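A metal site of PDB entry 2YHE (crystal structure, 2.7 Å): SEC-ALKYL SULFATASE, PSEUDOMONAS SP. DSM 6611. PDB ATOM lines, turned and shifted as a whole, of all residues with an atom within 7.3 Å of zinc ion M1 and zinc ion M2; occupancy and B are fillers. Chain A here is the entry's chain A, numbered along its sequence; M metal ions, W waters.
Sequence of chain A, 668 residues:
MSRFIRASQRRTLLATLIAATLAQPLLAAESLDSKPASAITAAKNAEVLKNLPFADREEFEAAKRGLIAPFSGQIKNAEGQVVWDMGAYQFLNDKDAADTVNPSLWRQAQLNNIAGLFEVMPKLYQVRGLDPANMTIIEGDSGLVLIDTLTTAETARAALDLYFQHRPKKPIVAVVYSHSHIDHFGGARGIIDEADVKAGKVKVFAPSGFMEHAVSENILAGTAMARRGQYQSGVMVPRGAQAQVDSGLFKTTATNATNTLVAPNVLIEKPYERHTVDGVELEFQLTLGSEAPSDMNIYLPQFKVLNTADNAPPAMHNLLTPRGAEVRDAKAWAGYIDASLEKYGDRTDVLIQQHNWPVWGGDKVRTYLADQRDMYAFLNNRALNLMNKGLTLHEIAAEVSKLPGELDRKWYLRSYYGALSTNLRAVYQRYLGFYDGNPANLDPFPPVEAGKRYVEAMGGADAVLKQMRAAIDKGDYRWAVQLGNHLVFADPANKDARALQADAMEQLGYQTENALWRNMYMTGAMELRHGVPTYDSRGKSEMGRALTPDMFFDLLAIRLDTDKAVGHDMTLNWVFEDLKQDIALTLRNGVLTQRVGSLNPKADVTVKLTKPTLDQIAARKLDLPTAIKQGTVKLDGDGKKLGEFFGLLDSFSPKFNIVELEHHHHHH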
ATOM      1  N   PRO A 132      22.170  16.861 -19.573  1.00  0.00           N
ATOM      2  CA  PRO A 132      21.473  16.119 -18.508  1.00  0.00           C
ATOM      3  C   PRO A 132      20.601  14.956 -19.055  1.00  0.00           C
ATOM      4  O   PRO A 132      20.591  13.855 -18.488  1.00  0.00           O
ATOM      5  CB  PRO A 132      20.584  17.166 -17.845  1.00  0.00           C
ATOM      6  CG  PRO A 132      21.283  18.436 -18.095  1.00  0.00           C
ATOM      7  CD  PRO A 132      21.930  18.306 -19.426  1.00  0.00           C
ATOM      8  N   ALA A 133      19.921  15.183 -20.191  1.00  0.00           N
ATOM      9  CA  ALA A 133      19.053  14.195 -20.836  1.00  0.00           C
ATOM     10  C   ALA A 133      19.734  13.471 -22.032  1.00  0.00           C
ATOM     11  O   ALA A 133      20.833  13.824 -22.427  1.00  0.00           O
ATOM     12  CB  ALA A 133      17.768  14.878 -21.288  1.00  0.00           C
ATOM     13  N   ASN A 134      19.062  12.466 -22.594  1.00  0.00           N
ATOM     14  CA  ASN A 134      19.509  11.716 -23.765  1.00  0.00           C
ATOM     15  C   ASN A 134      18.706  12.176 -24.988  1.00  0.00           C
ATOM     16  O   ASN A 134      17.616  12.750 -24.853  1.00  0.00           O
ATOM     17  CB  ASN A 134      19.273  10.199 -23.572  1.00  0.00           C
ATOM     18  CG  ASN A 134      20.032   9.560 -22.435  1.00  0.00           C
ATOM     19  OD1 ASN A 134      21.053  10.062 -21.969  1.00  0.00           O
ATOM     20  ND2 ASN A 134      19.547   8.409 -22.007  1.00  0.00           N
ATOM     21  N   ASP A 148      13.087  13.712 -28.338  1.00  0.00           N
ATOM     22  CA  ASP A 148      13.668  14.779 -27.515  1.00  0.00           C
ATOM     23  C   ASP A 148      14.849  15.490 -28.158  1.00  0.00           C
ATOM     24  O   ASP A 148      15.510  14.937 -29.037  1.00  0.00           O
ATOM     25  CB  ASP A 148      13.832  14.408 -26.034  1.00  0.00           C
ATOM     26  CG  ASP A 148      12.543  13.971 -25.343  1.00  0.00           C
ATOM     27  OD1 ASP A 148      11.477  14.498 -25.695  1.00  0.00           O
ATOM     28  OD2 ASP A 148      12.622  13.157 -24.416  1.00  0.00           O
ATOM     29  N   SER A 178       8.815  14.020 -25.411  1.00  0.00           N
ATOM     30  CA  SER A 178       8.244  12.971 -24.533  1.00  0.00           C
ATOM     31  C   SER A 178       7.473  13.565 -23.339  1.00  0.00           C
ATOM     32  O   SER A 178       6.482  12.982 -22.887  1.00  0.00           O
ATOM     33  CB  SER A 178       9.309  11.980 -24.096  1.00  0.00           C
ATOM     34  OG  SER A 178      10.227  12.522 -23.173  1.00  0.00           O
ATOM     35  N   HIS A 179       7.893  14.750 -22.876  1.00  0.00           N
ATOM     36  CA  HIS A 179       7.274  15.484 -21.785  1.00  0.00           C
ATOM     37  C   HIS A 179       7.677  16.959 -21.697  1.00  0.00           C
ATOM     38  O   HIS A 179       8.614  17.386 -22.384  1.00  0.00           O
ATOM     39  CB  HIS A 179       7.479  14.789 -20.435  1.00  0.00           C
ATOM     40  CG  HIS A 179       8.916  14.612 -20.025  1.00  0.00           C
ATOM     41  ND1 HIS A 179       9.765  13.745 -20.702  1.00  0.00           N
ATOM     42  CD2 HIS A 179       9.551  15.098 -18.937  1.00  0.00           C
ATOM     43  CE1 HIS A 179      10.887  13.764 -20.025  1.00  0.00           C
ATOM     44  NE2 HIS A 179      10.802  14.568 -18.955  1.00  0.00           N
ATOM     45  N   SER A 180       6.945  17.732 -20.837  1.00  0.00           N
ATOM     46  CA  SER A 180       7.091  19.184 -20.620  1.00  0.00           C
ATOM     47  C   SER A 180       8.275  19.607 -19.770  1.00  0.00           C
ATOM     48  O   SER A 180       8.201  20.603 -19.045  1.00  0.00           O
ATOM     49  CB  SER A 180       5.786  19.770 -20.115  1.00  0.00           C
ATOM     50  OG  SER A 180       5.306  19.118 -18.938  1.00  0.00           O
ATOM     51  N   HIS A 181       9.395  18.867 -19.857  1.00  0.00           N
ATOM     52  CA  HIS A 181      10.627  19.174 -19.121  1.00  0.00           C
ATOM     53  C   HIS A 181      11.689  19.805 -20.022  1.00  0.00           C
ATOM     54  O   HIS A 181      11.917  19.300 -21.129  1.00  0.00           O
ATOM     55  CB  HIS A 181      11.141  17.968 -18.342  1.00  0.00           C
ATOM     56  CG  HIS A 181      10.364  17.695 -17.067  1.00  0.00           C
ATOM     57  ND1 HIS A 181      10.591  16.560 -16.308  1.00  0.00           N
ATOM     58  CD2 HIS A 181       9.385  18.424 -16.483  1.00  0.00           C
ATOM     59  CE1 HIS A 181       9.760  16.646 -15.280  1.00  0.00           C
ATOM     60  NE2 HIS A 181       9.015  17.760 -15.346  1.00  0.00           N
ATOM     61  N   ILE A 182      12.292  20.918 -19.567  1.00  0.00           N
ATOM     62  CA  ILE A 182      13.331  21.680 -20.279  1.00  0.00           C
ATOM     63  C   ILE A 182      14.435  20.846 -20.865  1.00  0.00           C
ATOM     64  O   ILE A 182      14.906  21.179 -21.954  1.00  0.00           O
ATOM     65  CB  ILE A 182      13.948  22.887 -19.536  1.00  0.00           C
ATOM     66  CG1 ILE A 182      14.458  22.595 -18.112  1.00  0.00           C
ATOM     67  CG2 ILE A 182      13.211  24.149 -19.706  1.00  0.00           C
ATOM     68  CD1 ILE A 182      15.927  23.352 -17.809  1.00  0.00           C
ATOM     69  N   ASP A 183      14.834  19.741 -20.196  1.00  0.00           N
ATOM     70  CA  ASP A 183      15.897  18.848 -20.669  1.00  0.00           C
ATOM     71  C   ASP A 183      15.494  17.989 -21.898  1.00  0.00           C
ATOM     72  O   ASP A 183      16.298  17.195 -22.403  1.00  0.00           O
ATOM     73  CB  ASP A 183      16.490  18.028 -19.518  1.00  0.00           C
ATOM     74  CG  ASP A 183      15.505  17.281 -18.635  1.00  0.00           C
ATOM     75  OD1 ASP A 183      14.434  17.848 -18.319  1.00  0.00           O
ATOM     76  OD2 ASP A 183      15.807  16.127 -18.249  1.00  0.00           O
ATOM     77  N   HIS A 184      14.266  18.188 -22.404  1.00  0.00           N
ATOM     78  CA  HIS A 184      13.699  17.414 -23.494  1.00  0.00           C
ATOM     79  C   HIS A 184      13.235  18.269 -24.650  1.00  0.00           C
ATOM     80  O   HIS A 184      13.435  17.888 -25.806  1.00  0.00           O
ATOM     81  CB  HIS A 184      12.595  16.477 -22.935  1.00  0.00           C
ATOM     82  CG  HIS A 184      13.129  15.569 -21.863  1.00  0.00           C
ATOM     83  ND1 HIS A 184      13.628  14.308 -22.172  1.00  0.00           N
ATOM     84  CD2 HIS A 184      13.359  15.831 -20.559  1.00  0.00           C
ATOM     85  CE1 HIS A 184      14.101  13.822 -21.032  1.00  0.00           C
ATOM     86  NE2 HIS A 184      13.976  14.701 -20.030  1.00  0.00           N
ATOM     87  N   LEU A 249      20.814  11.105 -12.318  1.00  0.00           N
ATOM     88  CA  LEU A 249      20.294  10.786 -13.658  1.00  0.00           C
ATOM     89  C   LEU A 249      21.132  11.421 -14.740  1.00  0.00           C
ATOM     90  O   LEU A 249      20.887  11.220 -15.929  1.00  0.00           O
ATOM     91  CB  LEU A 249      18.819  11.206 -13.797  1.00  0.00           C
ATOM     92  CG  LEU A 249      17.793  10.512 -12.885  1.00  0.00           C
ATOM     93  CD1 LEU A 249      16.406  10.937 -13.256  1.00  0.00           C
ATOM     94  CD2 LEU A 249      17.927   8.987 -12.900  1.00  0.00           C
ATOM     95  N   PHE A 250      22.115  12.233 -14.319  1.00  0.00           N
ATOM     96  CA  PHE A 250      23.036  12.988 -15.186  1.00  0.00           C
ATOM     97  C   PHE A 250      24.158  13.525 -14.334  1.00  0.00           C
ATOM     98  O   PHE A 250      24.157  13.313 -13.100  1.00  0.00           O
ATOM     99  CB  PHE A 250      22.310  14.151 -15.876  1.00  0.00           C
ATOM    100  CG  PHE A 250      21.431  15.023 -15.003  1.00  0.00           C
ATOM    101  CD1 PHE A 250      20.103  14.702 -14.785  1.00  0.00           C
ATOM    102  CD2 PHE A 250      21.935  16.177 -14.437  1.00  0.00           C
ATOM    103  CE1 PHE A 250      19.296  15.502 -13.966  1.00  0.00           C
ATOM    104  CE2 PHE A 250      21.147  16.971 -13.610  1.00  0.00           C
ATOM    105  CZ  PHE A 250      19.831  16.621 -13.382  1.00  0.00           C
ATOM    106  N   GLU A 291       5.546  11.615 -14.009  1.00  0.00           N
ATOM    107  CA  GLU A 291       6.849  12.299 -13.962  1.00  0.00           C
ATOM    108  C   GLU A 291       6.789  13.806 -14.319  1.00  0.00           C
ATOM    109  O   GLU A 291       7.582  14.610 -13.823  1.00  0.00           O
ATOM    110  CB  GLU A 291       7.906  11.542 -14.803  1.00  0.00           C
ATOM    111  CG  GLU A 291       9.332  11.985 -14.531  1.00  0.00           C
ATOM    112  CD  GLU A 291       9.850  13.043 -15.491  1.00  0.00           C
ATOM    113  OE1 GLU A 291       9.195  13.261 -16.535  1.00  0.00           O
ATOM    114  OE2 GLU A 291      10.942  13.598 -15.228  1.00  0.00           O
ATOM    115  N   ALA A 292       5.853  14.175 -15.173  1.00  0.00           N
ATOM    116  CA  ALA A 292       5.653  15.552 -15.604  1.00  0.00           C
ATOM    117  C   ALA A 292       4.141  15.704 -15.851  1.00  0.00           C
ATOM    118  O   ALA A 292       3.465  14.703 -16.159  1.00  0.00           O
ATOM    119  CB  ALA A 292       6.457  15.837 -16.886  1.00  0.00           C
ATOM    120  N   ASP A 295       3.089  14.322 -20.200  1.00  0.00           N
ATOM    121  CA  ASP A 295       4.066  13.229 -20.276  1.00  0.00           C
ATOM    122  C   ASP A 295       3.546  12.008 -21.021  1.00  0.00           C
ATOM    123  O   ASP A 295       2.346  11.732 -20.990  1.00  0.00           O
ATOM    124  CB  ASP A 295       4.456  12.857 -18.832  1.00  0.00           C
ATOM    125  CG  ASP A 295       5.505  11.801 -18.618  1.00  0.00           C
ATOM    126  OD1 ASP A 295       6.334  11.574 -19.538  1.00  0.00           O
ATOM    127  OD2 ASP A 295       5.548  11.226 -17.501  1.00  0.00           O
ATOM    128  N   ALA A 309      10.572   7.302 -21.547  1.00  0.00           N
ATOM    129  CA  ALA A 309      10.890   8.713 -21.290  1.00  0.00           C
ATOM    130  C   ALA A 309      11.659   8.823 -19.954  1.00  0.00           C
ATOM    131  O   ALA A 309      12.724   8.225 -19.854  1.00  0.00           O
ATOM    132  CB  ALA A 309       9.612   9.561 -21.274  1.00  0.00           C
ATOM    133  N   ASP A 310      11.103   9.515 -18.935  1.00  0.00           N
ATOM    134  CA  ASP A 310      11.714   9.646 -17.603  1.00  0.00           C
ATOM    135  C   ASP A 310      10.828   8.961 -16.561  1.00  0.00           C
ATOM    136  O   ASP A 310      10.978   9.196 -15.363  1.00  0.00           O
ATOM    137  CB  ASP A 310      11.943  11.131 -17.208  1.00  0.00           C
ATOM    138  CG  ASP A 310      12.873  11.956 -18.084  1.00  0.00           C
ATOM    139  OD1 ASP A 310      13.295  11.450 -19.151  1.00  0.00           O
ATOM    140  OD2 ASP A 310      13.144  13.117 -17.715  1.00  0.00           O
ATOM    141  N   ASN A 311       9.923   8.104 -17.024  1.00  0.00           N
ATOM    142  CA  ASN A 311       8.953   7.402 -16.202  1.00  0.00           C
ATOM    143  C   ASN A 311       9.472   6.228 -15.434  1.00  0.00           C
ATOM    144  O   ASN A 311       8.865   5.853 -14.449  1.00  0.00           O
ATOM    145  CB  ASN A 311       7.732   7.035 -17.031  1.00  0.00           C
ATOM    146  CG  ASN A 311       7.027   8.244 -17.582  1.00  0.00           C
ATOM    147  OD1 ASN A 311       6.692   9.183 -16.842  1.00  0.00           O
ATOM    148  ND2 ASN A 311       6.834   8.267 -18.888  1.00  0.00           N
ATOM    149  N   HIS A 317      12.896   8.286  -8.797  1.00  0.00           N
ATOM    150  CA  HIS A 317      12.731   9.653  -9.295  1.00  0.00           C
ATOM    151  C   HIS A 317      12.044  10.519  -8.222  1.00  0.00           C
ATOM    152  O   HIS A 317      11.714  10.025  -7.132  1.00  0.00           O
ATOM    153  CB  HIS A 317      11.969   9.645 -10.621  1.00  0.00           C
ATOM    154  CG  HIS A 317      12.244  10.791 -11.551  1.00  0.00           C
ATOM    155  ND1 HIS A 317      12.500  12.068 -11.085  1.00  0.00           N
ATOM    156  CD2 HIS A 317      12.192  10.821 -12.899  1.00  0.00           C
ATOM    157  CE1 HIS A 317      12.596  12.823 -12.161  1.00  0.00           C
ATOM    158  NE2 HIS A 317      12.447  12.110 -13.277  1.00  0.00           N
ATOM    159  N   ARG A 323      14.011  21.707  -7.400  1.00  0.00           N
ATOM    160  CA  ARG A 323      13.960  22.972  -8.125  1.00  0.00           C
ATOM    161  C   ARG A 323      12.605  23.656  -8.010  1.00  0.00           C
ATOM    162  O   ARG A 323      12.514  24.877  -8.178  1.00  0.00           O
ATOM    163  CB  ARG A 323      14.348  22.779  -9.582  1.00  0.00           C
ATOM    164  CG  ARG A 323      13.397  21.914 -10.384  1.00  0.00           C
ATOM    165  CD  ARG A 323      13.997  21.490 -11.708  1.00  0.00           C
ATOM    166  NE  ARG A 323      13.178  20.444 -12.321  1.00  0.00           N
ATOM    167  CZ  ARG A 323      12.092  20.648 -13.055  1.00  0.00           C
ATOM    168  NH1 ARG A 323      11.653  21.893 -13.276  1.00  0.00           N
ATOM    169  NH2 ARG A 323      11.424  19.631 -13.561  1.00  0.00           N
ATOM    170  N   ARG A 328       3.771  15.270  -7.968  1.00  0.00           N
ATOM    171  CA  ARG A 328       3.558  14.191  -8.886  1.00  0.00           C
ATOM    172  C   ARG A 328       2.721  13.125  -8.217  1.00  0.00           C
ATOM    173  O   ARG A 328       2.735  12.989  -6.988  1.00  0.00           O
ATOM    174  CB  ARG A 328       4.938  13.688  -9.386  1.00  0.00           C
ATOM    175  CG  ARG A 328       5.627  14.801 -10.174  1.00  0.00           C
ATOM    176  CD  ARG A 328       7.078  14.610 -10.374  1.00  0.00           C
ATOM    177  NE  ARG A 328       7.662  15.759 -11.100  1.00  0.00           N
ATOM    178  CZ  ARG A 328       8.969  15.919 -11.329  1.00  0.00           C
ATOM    179  NH1 ARG A 328       9.842  14.993 -10.924  1.00  0.00           N
ATOM    180  NH2 ARG A 328       9.401  16.979 -11.985  1.00  0.00           N
ATOM    181  N   GLN A 354      15.113   8.378 -21.552  1.00  0.00           N
ATOM    182  CA  GLN A 354      15.608   9.702 -21.890  1.00  0.00           C
ATOM    183  C   GLN A 354      16.641  10.262 -20.869  1.00  0.00           C
ATOM    184  O   GLN A 354      17.074  11.415 -20.964  1.00  0.00           O
ATOM    185  CB  GLN A 354      14.463  10.653 -22.264  1.00  0.00           C
ATOM    186  CG  GLN A 354      13.685  10.194 -23.509  1.00  0.00           C
ATOM    187  CD  GLN A 354      14.534  10.084 -24.755  1.00  0.00           C
ATOM    188  OE1 GLN A 354      14.968   8.998 -25.151  1.00  0.00           O
ATOM    189  NE2 GLN A 354      14.785  11.203 -25.404  1.00  0.00           N
ATOM    190  N   HIS A 355      17.063   9.389 -19.936  1.00  0.00           N
ATOM    191  CA  HIS A 355      18.148   9.552 -18.969  1.00  0.00           C
ATOM    192  C   HIS A 355      18.719   8.169 -18.791  1.00  0.00           C
ATOM    193  O   HIS A 355      17.957   7.199 -18.798  1.00  0.00           O
ATOM    194  CB  HIS A 355      17.686  10.067 -17.595  1.00  0.00           C
ATOM    195  CG  HIS A 355      17.296  11.511 -17.617  1.00  0.00           C
ATOM    196  ND1 HIS A 355      18.242  12.529 -17.572  1.00  0.00           N
ATOM    197  CD2 HIS A 355      16.059  12.062 -17.690  1.00  0.00           C
ATOM    198  CE1 HIS A 355      17.540  13.652 -17.614  1.00  0.00           C
ATOM    199  NE2 HIS A 355      16.231  13.424 -17.683  1.00  0.00           N
ATOM    200  N   TYR A 417      18.418   9.992  -6.977  1.00  0.00           N
ATOM    201  CA  TYR A 417      17.778  11.190  -7.498  1.00  0.00           C
ATOM    202  C   TYR A 417      16.655  11.574  -6.531  1.00  0.00           C
ATOM    203  O   TYR A 417      16.823  12.495  -5.728  1.00  0.00           O
ATOM    204  CB  TYR A 417      17.261  10.926  -8.924  1.00  0.00           C
ATOM    205  CG  TYR A 417      17.071  12.180  -9.734  1.00  0.00           C
ATOM    206  CD1 TYR A 417      18.166  12.855 -10.269  1.00  0.00           C
ATOM    207  CD2 TYR A 417      15.802  12.669 -10.015  1.00  0.00           C
ATOM    208  CE1 TYR A 417      18.005  14.021 -11.020  1.00  0.00           C
ATOM    209  CE2 TYR A 417      15.623  13.850 -10.747  1.00  0.00           C
ATOM    210  CZ  TYR A 417      16.735  14.526 -11.239  1.00  0.00           C
ATOM    211  OH  TYR A 417      16.597  15.654 -12.001  1.00  0.00           O
HETATM  212 ZN    ZN M   1      11.581  14.702 -16.901  1.00  0.00          ZN
HETATM  213 ZN    ZN M   2      14.619  14.551 -18.184  1.00  0.00          ZN
HETATM  214  O   HOH W   1      13.875  15.240 -16.081  1.00  0.00           O
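ND1 of His 184 lies within hydrogen-bond range of OD2 of Asp 148 (2.7 Å).
A ring nitrogen (ND1) of His 355 lies within hydrogen-bond range of the backbone carbonyl oxygen of Pro 132, at 2.8 Å.
A ring nitrogen (ND1) of His 355 is in hydrogen-bond range of the backbone carbonyl oxygen (O) of Leu 249, 3.4 Å away.
The side-chain amide nitrogen (ND2) of Asn 134 sits close to the backbone NH (N) of His 355, 3.4 Å away.
A ring nitrogen (NE2) of His 317 lies close to the side-chain carboxylate of Glu 291 (2.9 Å).
The backbone carbonyl oxygen (O) of Glu 291 is in hydrogen-bond range of the guanidinium group (NE) of Arg 328 (3.0 Å).
NE2 of His 181 lies close to NH2 of Arg 328, 3.5 Å away.
A ring nitrogen (ND1) of His 179 is in hydrogen-bond range of the side-chain hydroxyl of Ser 178 (2.8 Å).
Five residues have an atom within 4 Å of zinc ion M1: His 179, His 181, His 184, Glu 291 and Asp 310.
Of the 25 residues printed, 5 come within 4 Å of zinc ion M2.
The nearest printed residue that does not touch zinc ion M2 is Ala 133 (4.4 Å).
Zinc ion M1 is bound by OE2 of Glu 291 (2.1 Å), ND1 of His 181 (2.2 Å), NE2 of His 179 (2.2 Å), OD2 of Asp 310 (2.4 Å) and water W1 (2.5 Å).
Slightly farther from zinc ion M1 lies OE1 of Glu 291 (2.8 Å).
Zinc ion M2 is bound by NE2 of His 184 (2.0 Å), OD2 of Asp 183 (2.0 Å), NE2 of His 355 (2.0 Å), OD2 of Asp 310 (2.1 Å) and water W1 (2.3 Å).
Zinc ion M2 has five donor atoms within binding distance.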
